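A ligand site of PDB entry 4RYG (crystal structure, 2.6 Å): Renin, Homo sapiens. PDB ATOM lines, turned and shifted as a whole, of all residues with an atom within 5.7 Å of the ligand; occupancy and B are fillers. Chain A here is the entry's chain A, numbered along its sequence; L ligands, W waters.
An oxygen (O1) of the ligand lies within hydrogen-bond range of the side-chain hydroxyl (OG1) of Thr 85 (2.7 Å). OD1 of Asp 38 is in salt-bridge range of N3 of the ligand (2.8 Å). OD2 of Asp 226 is in salt-bridge range of N3 of the ligand (2.8 Å). N of Tyr 20 lies within hydrogen-bond range of O4 of the ligand (3.1 Å). The backbone NH of Ser 84 is in hydrogen-bond range of an oxygen (O6) of the ligand, at 3.3 Å.
OD2 of Asp 38 lies within hydrogen-bond range of OG of Ser 41. The backbone NH (N) of Gly 40 sits at hydrogen-bond distance from the side-chain carboxylate (OD1) of Asp 226 (3.3 Å). The backbone NH (N) of Ala 317 sits at hydrogen-bond distance from the backbone carbonyl oxygen (O) of Ser 230, at 3.5 Å. The indole nitrogen (NE1) of Trp 45 is in hydrogen-bond range of the side-chain hydroxyl (OH) of Tyr 83. The side-chain amide nitrogen (NE2) of Gln 19 is in hydrogen-bond range of the backbone carbonyl oxygen (O) of Leu 121, 2.9 Å away. OG1 of Thr 227 sits at hydrogen-bond distance from N of Thr 39, 2.8 Å away. The backbone NH of Val 127 lies within hydrogen-bond range of the backbone carbonyl oxygen of Trp 45. The side-chain hydroxyl (OG1) of Thr 309 is in hydrogen-bond range of the side-chain amide oxygen (OE1) of Gln 135, at 3.3 Å.
The backbone carbonyl oxygen (O) of Thr 18 lies close to an oxygen (O4) of the ligand (3.4 Å). CA of Gln 19 touches O4 of the ligand, at 3.5 Å. CG1 of Val 36 touches C13 of the ligand, at 3.7 Å. Gly 40 touches the ligand (O to C9, 3.4 Å). CA of Tyr 83 touches O6 of the ligand (3.4 Å). Pro 118 touches the ligand. CB of Leu 121 touches C18 of the ligand, 3.8 Å away. N of Ala 122 touches C18 of the ligand, at 3.9 Å. Phe 124 touches the ligand. Val 127 touches the ligand (CG2 to C15, 3.6 Å). CD2 of Leu 224 touches C26 of the ligand, 3.7 Å away. Thr 227 touches the ligand. O of Gly 228 touches C13 of the ligand, at 3.3 Å. O of Ala 229 touches C24 of the ligand (3.4 Å). Ser 230 touches the ligand. Met 303 touches the ligand (SD to O5, 3.96 Å). CG1 of Ile 305 touches C3 of the ligand, 3.6 Å away. Thr 309 touches the ligand. Ala 317 touches the ligand (CB to C24, 3.9 Å). Hydrophobic or aromatic side chains that line the ligand: Tyr 20, Val 36, Tyr 83, Pro 118, Leu 121, Phe 124, Val 127, Leu 224, Met 303, Ile 305 and Ala 317. The nearest printed residue that does not touch the ligand is Ser 41 (4.2 Å).
Water W2 bridges O2 of the ligand (2.9 Å) and OG of Ser 230 (2.9 Å).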
ATOM      1  N   THR A  18      -2.998  -0.410  12.493  1.00  0.00           N
ATOM      2  CA  THR A  18      -3.744  -1.649  12.725  1.00  0.00           C
ATOM      3  C   THR A  18      -4.782  -1.554  13.841  1.00  0.00           C
ATOM      4  O   THR A  18      -5.780  -2.257  13.781  1.00  0.00           O
ATOM      5  CB  THR A  18      -2.826  -2.835  13.005  1.00  0.00           C
ATOM      6  OG1 THR A  18      -1.995  -2.574  14.142  1.00  0.00           O
ATOM      7  CG2 THR A  18      -2.012  -3.220  11.831  1.00  0.00           C
ATOM      8  N   GLN A  19      -4.559  -0.727  14.863  1.00  0.00           N
ATOM      9  CA  GLN A  19      -5.504  -0.612  15.986  1.00  0.00           C
ATOM     10  C   GLN A  19      -5.863   0.837  16.195  1.00  0.00           C
ATOM     11  O   GLN A  19      -4.952   1.653  16.304  1.00  0.00           O
ATOM     12  CB  GLN A  19      -4.899  -1.198  17.272  1.00  0.00           C
ATOM     13  CG  GLN A  19      -4.463  -2.664  17.147  1.00  0.00           C
ATOM     14  CD  GLN A  19      -3.816  -3.214  18.382  1.00  0.00           C
ATOM     15  OE1 GLN A  19      -4.190  -2.854  19.495  1.00  0.00           O
ATOM     16  NE2 GLN A  19      -2.839  -4.110  18.211  1.00  0.00           N
ATOM     17  N   TYR A  20      -7.187   1.166  16.252  1.00  0.00           N
ATOM     18  CA  TYR A  20      -7.715   2.525  16.501  1.00  0.00           C
ATOM     19  C   TYR A  20      -8.577   2.462  17.718  1.00  0.00           C
ATOM     20  O   TYR A  20      -9.543   1.687  17.784  1.00  0.00           O
ATOM     21  CB  TYR A  20      -8.521   3.037  15.317  1.00  0.00           C
ATOM     22  CG  TYR A  20      -7.692   3.306  14.086  1.00  0.00           C
ATOM     23  CD1 TYR A  20      -7.279   2.260  13.265  1.00  0.00           C
ATOM     24  CD2 TYR A  20      -7.326   4.602  13.740  1.00  0.00           C
ATOM     25  CE1 TYR A  20      -6.508   2.506  12.133  1.00  0.00           C
ATOM     26  CE2 TYR A  20      -6.560   4.864  12.606  1.00  0.00           C
ATOM     27  CZ  TYR A  20      -6.162   3.799  11.802  1.00  0.00           C
ATOM     28  OH  TYR A  20      -5.440   4.031  10.665  1.00  0.00           O
ATOM     29  N   VAL A  36     -11.963  -0.245  21.585  1.00  0.00           N
ATOM     30  CA  VAL A  36     -12.168  -0.253  20.148  1.00  0.00           C
ATOM     31  C   VAL A  36     -13.685  -0.037  19.938  1.00  0.00           C
ATOM     32  O   VAL A  36     -14.509  -0.702  20.586  1.00  0.00           O
ATOM     33  CB  VAL A  36     -11.685  -1.588  19.531  1.00  0.00           C
ATOM     34  CG1 VAL A  36     -12.250  -1.787  18.127  1.00  0.00           C
ATOM     35  CG2 VAL A  36     -10.163  -1.654  19.514  1.00  0.00           C
ATOM     36  N   ASP A  38     -16.351  -0.770  17.690  1.00  0.00           N
ATOM     37  CA  ASP A  38     -16.501  -1.855  16.713  1.00  0.00           C
ATOM     38  C   ASP A  38     -17.922  -2.030  16.162  1.00  0.00           C
ATOM     39  O   ASP A  38     -18.794  -2.445  16.904  1.00  0.00           O
ATOM     40  CB  ASP A  38     -15.979  -3.170  17.345  1.00  0.00           C
ATOM     41  CG  ASP A  38     -16.157  -4.420  16.525  1.00  0.00           C
ATOM     42  OD1 ASP A  38     -16.287  -4.300  15.293  1.00  0.00           O
ATOM     43  OD2 ASP A  38     -16.125  -5.518  17.120  1.00  0.00           O
ATOM     44  N   THR A  39     -18.129  -1.734  14.868  1.00  0.00           N
ATOM     45  CA  THR A  39     -19.430  -1.848  14.197  1.00  0.00           C
ATOM     46  C   THR A  39     -19.773  -3.313  13.838  1.00  0.00           C
ATOM     47  O   THR A  39     -20.917  -3.624  13.497  1.00  0.00           O
ATOM     48  CB  THR A  39     -19.558  -0.911  12.993  1.00  0.00           C
ATOM     49  OG1 THR A  39     -18.461  -1.134  12.084  1.00  0.00           O
ATOM     50  CG2 THR A  39     -19.641   0.546  13.404  1.00  0.00           C
ATOM     51  N   GLY A  40     -18.790  -4.193  13.952  1.00  0.00           N
ATOM     52  CA  GLY A  40     -18.939  -5.617  13.707  1.00  0.00           C
ATOM     53  C   GLY A  40     -19.454  -6.387  14.905  1.00  0.00           C
ATOM     54  O   GLY A  40     -19.644  -7.590  14.796  1.00  0.00           O
ATOM     55  N   SER A  41     -19.655  -5.721  16.064  1.00  0.00           N
ATOM     56  CA  SER A  41     -20.138  -6.351  17.312  1.00  0.00           C
ATOM     57  C   SER A  41     -21.032  -5.396  18.124  1.00  0.00           C
ATOM     58  O   SER A  41     -21.034  -4.198  17.860  1.00  0.00           O
ATOM     59  CB  SER A  41     -18.979  -6.915  18.134  1.00  0.00           C
ATOM     60  OG  SER A  41     -18.201  -5.892  18.745  1.00  0.00           O
ATOM     61  N   TRP A  45     -17.416  -4.542  26.590  1.00  0.00           N
ATOM     62  CA  TRP A  45     -16.672  -5.362  27.544  1.00  0.00           C
ATOM     63  C   TRP A  45     -15.311  -4.775  27.834  1.00  0.00           C
ATOM     64  O   TRP A  45     -14.693  -4.182  26.944  1.00  0.00           O
ATOM     65  CB  TRP A  45     -16.579  -6.827  27.092  1.00  0.00           C
ATOM     66  CG  TRP A  45     -15.649  -7.099  25.941  1.00  0.00           C
ATOM     67  CD1 TRP A  45     -16.004  -7.356  24.643  1.00  0.00           C
ATOM     68  CD2 TRP A  45     -14.226  -7.297  26.014  1.00  0.00           C
ATOM     69  NE1 TRP A  45     -14.883  -7.673  23.912  1.00  0.00           N
ATOM     70  CE2 TRP A  45     -13.782  -7.617  24.716  1.00  0.00           C
ATOM     71  CE3 TRP A  45     -13.281  -7.233  27.054  1.00  0.00           C
ATOM     72  CZ2 TRP A  45     -12.436  -7.834  24.432  1.00  0.00           C
ATOM     73  CZ3 TRP A  45     -11.950  -7.449  26.763  1.00  0.00           C
ATOM     74  CH2 TRP A  45     -11.538  -7.759  25.467  1.00  0.00           C
ATOM     75  N   ARG A  82     -17.577 -14.977  21.304  1.00  0.00           N
ATOM     76  CA  ARG A  82     -16.746 -15.763  20.375  1.00  0.00           C
ATOM     77  C   ARG A  82     -16.435 -14.990  19.111  1.00  0.00           C
ATOM     78  O   ARG A  82     -17.145 -15.058  18.104  1.00  0.00           O
ATOM     79  CB  ARG A  82     -17.380 -17.120  20.028  1.00  0.00           C
ATOM     80  CG  ARG A  82     -17.067 -18.238  20.994  1.00  0.00           C
ATOM     81  CD  ARG A  82     -18.049 -19.394  20.828  1.00  0.00           C
ATOM     82  NE  ARG A  82     -18.261 -20.130  22.071  1.00  0.00           N
ATOM     83  CZ  ARG A  82     -19.342 -20.032  22.842  1.00  0.00           C
ATOM     84  NH1 ARG A  82     -20.344 -19.234  22.485  1.00  0.00           N
ATOM     85  NH2 ARG A  82     -19.448 -20.748  23.960  1.00  0.00           N
ATOM     86  N   TYR A  83     -15.380 -14.217  19.178  1.00  0.00           N
ATOM     87  CA  TYR A  83     -14.913 -13.542  17.992  1.00  0.00           C
ATOM     88  C   TYR A  83     -14.074 -14.615  17.287  1.00  0.00           C
ATOM     89  O   TYR A  83     -13.495 -15.516  17.925  1.00  0.00           O
ATOM     90  CB  TYR A  83     -14.065 -12.302  18.333  1.00  0.00           C
ATOM     91  CG  TYR A  83     -14.740 -11.277  19.232  1.00  0.00           C
ATOM     92  CD1 TYR A  83     -15.731 -10.436  18.742  1.00  0.00           C
ATOM     93  CD2 TYR A  83     -14.335 -11.089  20.550  1.00  0.00           C
ATOM     94  CE1 TYR A  83     -16.321  -9.459  19.546  1.00  0.00           C
ATOM     95  CE2 TYR A  83     -14.912 -10.125  21.367  1.00  0.00           C
ATOM     96  CZ  TYR A  83     -15.901  -9.304  20.855  1.00  0.00           C
ATOM     97  OH  TYR A  83     -16.485  -8.339  21.639  1.00  0.00           O
ATOM     98  N   SER A  84     -14.071 -14.545  15.979  1.00  0.00           N
ATOM     99  CA  SER A  84     -13.386 -15.480  15.098  1.00  0.00           C
ATOM    100  C   SER A  84     -11.847 -15.266  15.125  1.00  0.00           C
ATOM    101  O   SER A  84     -11.086 -16.058  14.526  1.00  0.00           O
ATOM    102  CB  SER A  84     -13.977 -15.343  13.697  1.00  0.00           C
ATOM    103  OG  SER A  84     -15.400 -15.437  13.663  1.00  0.00           O
ATOM    104  N   THR A  85     -11.402 -14.216  15.824  1.00  0.00           N
ATOM    105  CA  THR A  85      -9.969 -13.901  16.036  1.00  0.00           C
ATOM    106  C   THR A  85      -9.493 -14.505  17.363  1.00  0.00           C
ATOM    107  O   THR A  85      -8.288 -14.755  17.555  1.00  0.00           O
ATOM    108  CB  THR A  85      -9.755 -12.376  16.116  1.00  0.00           C
ATOM    109  OG1 THR A  85     -11.008 -11.707  16.230  1.00  0.00           O
ATOM    110  CG2 THR A  85      -8.938 -11.837  14.955  1.00  0.00           C
ATOM    111  N   PRO A 118      -5.396 -13.130  20.857  1.00  0.00           N
ATOM    112  CA  PRO A 118      -4.550 -12.016  20.406  1.00  0.00           C
ATOM    113  C   PRO A 118      -4.356 -10.847  21.377  1.00  0.00           C
ATOM    114  O   PRO A 118      -3.650  -9.911  21.016  1.00  0.00           O
ATOM    115  CB  PRO A 118      -5.327 -11.537  19.173  1.00  0.00           C
ATOM    116  CG  PRO A 118      -6.778 -11.681  19.607  1.00  0.00           C
ATOM    117  CD  PRO A 118      -6.812 -12.880  20.542  1.00  0.00           C
ATOM    118  N   PHE A 119      -4.943 -10.895  22.590  1.00  0.00           N
ATOM    119  CA  PHE A 119      -4.971  -9.772  23.533  1.00  0.00           C
ATOM    120  C   PHE A 119      -3.614  -9.319  24.080  1.00  0.00           C
ATOM    121  O   PHE A 119      -3.520  -8.182  24.487  1.00  0.00           O
ATOM    122  CB  PHE A 119      -6.006 -10.008  24.644  1.00  0.00           C
ATOM    123  CG  PHE A 119      -7.359 -10.218  23.998  1.00  0.00           C
ATOM    124  CD1 PHE A 119      -8.007  -9.174  23.348  1.00  0.00           C
ATOM    125  CD2 PHE A 119      -7.917 -11.485  23.895  1.00  0.00           C
ATOM    126  CE1 PHE A 119      -9.203  -9.387  22.666  1.00  0.00           C
ATOM    127  CE2 PHE A 119      -9.103 -11.698  23.187  1.00  0.00           C
ATOM    128  CZ  PHE A 119      -9.742 -10.651  22.593  1.00  0.00           C
ATOM    129  N   LEU A 121      -1.208  -8.704  22.145  1.00  0.00           N
ATOM    130  CA  LEU A 121      -0.872  -7.823  21.019  1.00  0.00           C
ATOM    131  C   LEU A 121      -1.779  -6.622  21.011  1.00  0.00           C
ATOM    132  O   LEU A 121      -1.533  -5.670  20.260  1.00  0.00           O
ATOM    133  CB  LEU A 121      -1.045  -8.558  19.682  1.00  0.00           C
ATOM    134  CG  LEU A 121      -0.484  -9.965  19.515  1.00  0.00           C
ATOM    135  CD1 LEU A 121      -1.268 -10.719  18.429  1.00  0.00           C
ATOM    136  CD2 LEU A 121       1.024  -9.953  19.264  1.00  0.00           C
ATOM    137  N   ALA A 122      -2.874  -6.658  21.800  1.00  0.00           N
ATOM    138  CA  ALA A 122      -3.848  -5.574  21.879  1.00  0.00           C
ATOM    139  C   ALA A 122      -3.293  -4.367  22.683  1.00  0.00           C
ATOM    140  O   ALA A 122      -2.803  -4.552  23.800  1.00  0.00           O
ATOM    141  CB  ALA A 122      -5.159  -6.063  22.493  1.00  0.00           C
ATOM    142  N   PHE A 124      -5.413  -1.771  23.083  1.00  0.00           N
ATOM    143  CA  PHE A 124      -6.689  -1.445  23.738  1.00  0.00           C
ATOM    144  C   PHE A 124      -6.936  -2.468  24.823  1.00  0.00           C
ATOM    145  O   PHE A 124      -6.414  -3.588  24.731  1.00  0.00           O
ATOM    146  CB  PHE A 124      -7.854  -1.491  22.703  1.00  0.00           C
ATOM    147  CG  PHE A 124      -7.982  -2.788  21.926  1.00  0.00           C
ATOM    148  CD1 PHE A 124      -7.172  -3.052  20.826  1.00  0.00           C
ATOM    149  CD2 PHE A 124      -8.936  -3.745  22.280  1.00  0.00           C
ATOM    150  CE1 PHE A 124      -7.308  -4.231  20.099  1.00  0.00           C
ATOM    151  CE2 PHE A 124      -9.064  -4.929  21.548  1.00  0.00           C
ATOM    152  CZ  PHE A 124      -8.258  -5.168  20.462  1.00  0.00           C
ATOM    153  N   VAL A 127     -13.652  -3.464  24.326  1.00  0.00           N
ATOM    154  CA  VAL A 127     -14.436  -3.202  23.114  1.00  0.00           C
ATOM    155  C   VAL A 127     -15.752  -2.533  23.432  1.00  0.00           C
ATOM    156  O   VAL A 127     -16.409  -2.893  24.404  1.00  0.00           O
ATOM    157  CB  VAL A 127     -14.663  -4.544  22.343  1.00  0.00           C
ATOM    158  CG1 VAL A 127     -15.475  -4.341  21.052  1.00  0.00           C
ATOM    159  CG2 VAL A 127     -13.345  -5.270  22.042  1.00  0.00           C
ATOM    160  N   GLN A 135     -27.506  -8.499  17.259  1.00  0.00           N
ATOM    161  CA  GLN A 135     -26.227  -9.220  17.308  1.00  0.00           C
ATOM    162  C   GLN A 135     -25.590  -9.188  18.711  1.00  0.00           C
ATOM    163  O   GLN A 135     -24.446  -9.626  18.872  1.00  0.00           O
ATOM    164  CB  GLN A 135     -25.250  -8.707  16.226  1.00  0.00           C
ATOM    165  CG  GLN A 135     -25.734  -8.877  14.778  1.00  0.00           C
ATOM    166  CD  GLN A 135     -25.709 -10.314  14.268  1.00  0.00           C
ATOM    167  OE1 GLN A 135     -24.648 -10.884  13.993  1.00  0.00           O
ATOM    168  NE2 GLN A 135     -26.887 -10.894  14.067  1.00  0.00           N
ATOM    169  N   TYR A 162     -10.530   7.597  10.297  1.00  0.00           N
ATOM    170  CA  TYR A 162      -9.299   6.885  10.653  1.00  0.00           C
ATOM    171  C   TYR A 162      -8.199   7.515   9.826  1.00  0.00           C
ATOM    172  O   TYR A 162      -8.283   7.485   8.597  1.00  0.00           O
ATOM    173  CB  TYR A 162      -9.388   5.387  10.296  1.00  0.00           C
ATOM    174  CG  TYR A 162     -10.131   4.484  11.252  1.00  0.00           C
ATOM    175  CD1 TYR A 162     -10.666   4.978  12.445  1.00  0.00           C
ATOM    176  CD2 TYR A 162     -10.279   3.130  10.984  1.00  0.00           C
ATOM    177  CE1 TYR A 162     -11.336   4.147  13.322  1.00  0.00           C
ATOM    178  CE2 TYR A 162     -10.953   2.287  11.868  1.00  0.00           C
ATOM    179  CZ  TYR A 162     -11.466   2.796  13.040  1.00  0.00           C
ATOM    180  OH  TYR A 162     -12.099   1.963  13.917  1.00  0.00           O
ATOM    181  N   LEU A 224     -19.477  -6.466   5.000  1.00  0.00           N
ATOM    182  CA  LEU A 224     -19.665  -6.001   6.377  1.00  0.00           C
ATOM    183  C   LEU A 224     -18.729  -4.786   6.541  1.00  0.00           C
ATOM    184  O   LEU A 224     -17.540  -4.884   6.200  1.00  0.00           O
ATOM    185  CB  LEU A 224     -19.331  -7.120   7.383  1.00  0.00           C
ATOM    186  CG  LEU A 224     -19.369  -6.733   8.873  1.00  0.00           C
ATOM    187  CD1 LEU A 224     -20.812  -6.503   9.401  1.00  0.00           C
ATOM    188  CD2 LEU A 224     -18.607  -7.761   9.706  1.00  0.00           C
ATOM    189  N   ASP A 226     -16.924  -2.876   8.928  1.00  0.00           N
ATOM    190  CA  ASP A 226     -16.400  -3.172  10.257  1.00  0.00           C
ATOM    191  C   ASP A 226     -15.241  -2.268  10.754  1.00  0.00           C
ATOM    192  O   ASP A 226     -14.065  -2.505  10.440  1.00  0.00           O
ATOM    193  CB  ASP A 226     -15.958  -4.641  10.256  1.00  0.00           C
ATOM    194  CG  ASP A 226     -15.681  -5.277  11.579  1.00  0.00           C
ATOM    195  OD1 ASP A 226     -15.840  -4.594  12.617  1.00  0.00           O
ATOM    196  OD2 ASP A 226     -15.358  -6.499  11.599  1.00  0.00           O
ATOM    197  N   THR A 227     -15.578  -1.317  11.621  1.00  0.00           N
ATOM    198  CA  THR A 227     -14.615  -0.389  12.222  1.00  0.00           C
ATOM    199  C   THR A 227     -13.587  -1.091  13.152  1.00  0.00           C
ATOM    200  O   THR A 227     -12.470  -0.585  13.322  1.00  0.00           O
ATOM    201  CB  THR A 227     -15.358   0.699  12.987  1.00  0.00           C
ATOM    202  OG1 THR A 227     -16.116   0.078  14.020  1.00  0.00           O
ATOM    203  CG2 THR A 227     -16.283   1.552  12.068  1.00  0.00           C
ATOM    204  N   GLY A 228     -13.960  -2.243  13.724  1.00  0.00           N
ATOM    205  CA  GLY A 228     -13.125  -3.006  14.646  1.00  0.00           C
ATOM    206  C   GLY A 228     -12.161  -3.966  13.983  1.00  0.00           C
ATOM    207  O   GLY A 228     -11.439  -4.695  14.677  1.00  0.00           O
ATOM    208  N   ALA A 229     -12.136  -3.996  12.653  1.00  0.00           N
ATOM    209  CA  ALA A 229     -11.257  -4.865  11.888  1.00  0.00           C
ATOM    210  C   ALA A 229     -10.133  -4.012  11.328  1.00  0.00           C
ATOM    211  O   ALA A 229     -10.366  -2.854  10.949  1.00  0.00           O
ATOM    212  CB  ALA A 229     -12.030  -5.549  10.753  1.00  0.00           C
ATOM    213  N   SER A 230      -8.927  -4.573  11.316  1.00  0.00           N
ATOM    214  CA  SER A 230      -7.754  -3.867  10.830  1.00  0.00           C
ATOM    215  C   SER A 230      -7.696  -3.846   9.331  1.00  0.00           C
ATOM    216  O   SER A 230      -7.246  -2.853   8.760  1.00  0.00           O
ATOM    217  CB  SER A 230      -6.479  -4.538  11.333  1.00  0.00           C
ATOM    218  OG  SER A 230      -6.448  -4.623  12.739  1.00  0.00           O
ATOM    219  N   MET A 303     -10.546 -14.256   5.888  1.00  0.00           N
ATOM    220  CA  MET A 303     -11.381 -14.454   7.064  1.00  0.00           C
ATOM    221  C   MET A 303     -12.742 -14.979   6.690  1.00  0.00           C
ATOM    222  O   MET A 303     -13.513 -14.317   6.000  1.00  0.00           O
ATOM    223  CB  MET A 303     -11.469 -13.238   7.968  1.00  0.00           C
ATOM    224  CG  MET A 303     -11.542 -13.657   9.387  1.00  0.00           C
ATOM    225  SD  MET A 303     -12.002 -12.319  10.462  1.00  0.00           S
ATOM    226  CE  MET A 303     -10.404 -11.651  10.838  1.00  0.00           C
ATOM    227  N   ILE A 305     -16.027 -15.604   7.849  1.00  0.00           N
ATOM    228  CA  ILE A 305     -17.010 -15.188   8.856  1.00  0.00           C
ATOM    229  C   ILE A 305     -18.142 -16.201   8.713  1.00  0.00           C
ATOM    230  O   ILE A 305     -18.561 -16.474   7.588  1.00  0.00           O
ATOM    231  CB  ILE A 305     -17.453 -13.700   8.659  1.00  0.00           C
ATOM    232  CG1 ILE A 305     -16.297 -12.728   9.017  1.00  0.00           C
ATOM    233  CG2 ILE A 305     -18.719 -13.356   9.447  1.00  0.00           C
ATOM    234  CD1 ILE A 305     -15.982 -11.680   7.982  1.00  0.00           C
ATOM    235  N   PRO A 306     -18.569 -16.819   9.824  1.00  0.00           N
ATOM    236  CA  PRO A 306     -19.629 -17.849   9.732  1.00  0.00           C
ATOM    237  C   PRO A 306     -21.023 -17.294   9.448  1.00  0.00           C
ATOM    238  O   PRO A 306     -21.287 -16.121   9.758  1.00  0.00           O
ATOM    239  CB  PRO A 306     -19.590 -18.494  11.120  1.00  0.00           C
ATOM    240  CG  PRO A 306     -19.130 -17.399  12.023  1.00  0.00           C
ATOM    241  CD  PRO A 306     -18.122 -16.622  11.227  1.00  0.00           C
ATOM    242  N   THR A 309     -24.343 -14.083   9.308  1.00  0.00           N
ATOM    243  CA  THR A 309     -23.626 -12.901   8.813  1.00  0.00           C
ATOM    244  C   THR A 309     -22.775 -13.242   7.570  1.00  0.00           C
ATOM    245  O   THR A 309     -22.901 -12.573   6.543  1.00  0.00           O
ATOM    246  CB  THR A 309     -22.820 -12.218   9.961  1.00  0.00           C
ATOM    247  OG1 THR A 309     -23.709 -11.873  11.021  1.00  0.00           O
ATOM    248  CG2 THR A 309     -22.094 -10.963   9.500  1.00  0.00           C
ATOM    249  N   ALA A 317     -10.256  -1.082   8.718  1.00  0.00           N
ATOM    250  CA  ALA A 317      -9.513   0.197   8.751  1.00  0.00           C
ATOM    251  C   ALA A 317      -8.812   0.535   7.430  1.00  0.00           C
ATOM    252  O   ALA A 317      -8.682   1.719   7.143  1.00  0.00           O
ATOM    253  CB  ALA A 317      -8.546   0.233   9.920  1.00  0.00           C
HETATM  254  C1  LIG L   1     -10.893  -8.317  16.583  1.00  0.00           C
HETATM  255  C2  LIG L   1     -13.381  -8.347  16.870  1.00  0.00           C
HETATM  256  C3  LIG L   1     -15.720 -11.814  12.502  1.00  0.00           C
HETATM  257  C4  LIG L   1      -6.843  -7.119  17.722  1.00  0.00           C
HETATM  258  C5  LIG L   1      -8.685  -8.735  17.808  1.00  0.00           C
HETATM  259  C6  LIG L   1     -11.874  -7.015  18.441  1.00  0.00           C
HETATM  260  C7  LIG L   1      -7.399  -8.338  18.197  1.00  0.00           C
HETATM  261  C8  LIG L   1     -14.061  -6.793  14.842  1.00  0.00           C
HETATM  262  C9  LIG L   1     -16.210  -7.859  14.949  1.00  0.00           C
HETATM  263  C10 LIG L   1     -17.245 -11.618  12.608  1.00  0.00           C
HETATM  264  C11 LIG L   1      -8.597  -3.094  16.513  1.00  0.00           C
HETATM  265  C12 LIG L   1      -7.813  -4.091  15.641  1.00  0.00           C
HETATM  266  C13 LIG L   1      -9.550  -2.192  15.672  1.00  0.00           C
HETATM  267  C14 LIG L   1     -12.520  -5.603  18.322  1.00  0.00           C
HETATM  268  C15 LIG L   1     -12.143  -7.770  19.760  1.00  0.00           C
HETATM  269  C16 LIG L   1     -18.081 -12.687  13.010  1.00  0.00           C
HETATM  270  C17 LIG L   1     -17.806 -10.379  12.297  1.00  0.00           C
HETATM  271  C18 LIG L   1      -4.407  -7.562  18.277  1.00  0.00           C
HETATM  272  N1  LIG L   1     -12.030  -7.867  17.247  1.00  0.00           N
HETATM  273  C19 LIG L   1     -13.831  -8.203  15.396  1.00  0.00           C
HETATM  274  N2  LIG L   1     -15.047  -9.785  13.950  1.00  0.00           N
HETATM  275  C20 LIG L   1      -9.481  -7.914  16.985  1.00  0.00           C
HETATM  276  C21 LIG L   1     -15.149  -8.952  15.117  1.00  0.00           C
HETATM  277  C22 LIG L   1      -8.958  -6.702  16.527  1.00  0.00           C
HETATM  278  C23 LIG L   1      -7.639  -6.282  16.884  1.00  0.00           C
HETATM  279  N3  LIG L   1     -15.446  -6.746  14.358  1.00  0.00           N
HETATM  280  O1  LIG L   1     -10.908  -9.057  15.613  1.00  0.00           O
HETATM  281  O2  LIG L   1      -7.088  -5.055  16.437  1.00  0.00           O
HETATM  282  O3  LIG L   1      -5.535  -6.690  18.075  1.00  0.00           O
HETATM  283  O4  LIG L   1      -8.815  -1.162  15.002  1.00  0.00           O
HETATM  284  C24 LIG L   1      -9.023  -1.183  13.572  1.00  0.00           C
HETATM  285  C25 LIG L   1     -19.472 -12.526  13.071  1.00  0.00           C
HETATM  286  C26 LIG L   1     -19.204 -10.206  12.378  1.00  0.00           C
HETATM  287  C27 LIG L   1     -20.035 -11.283  12.751  1.00  0.00           C
HETATM  288  S1  LIG L   1     -14.956 -11.406  14.092  1.00  0.00           S
HETATM  289  O5  LIG L   1     -13.544 -11.745  14.062  1.00  0.00           O
HETATM  290  O6  LIG L   1     -15.767 -11.882  15.201  1.00  0.00           O
HETATM  291  O   HOH W   1     -18.560 -10.680  16.313  1.00  0.00           O
HETATM  292  O   HOH W   2      -5.060  -6.190  14.737  1.00  0.00           O
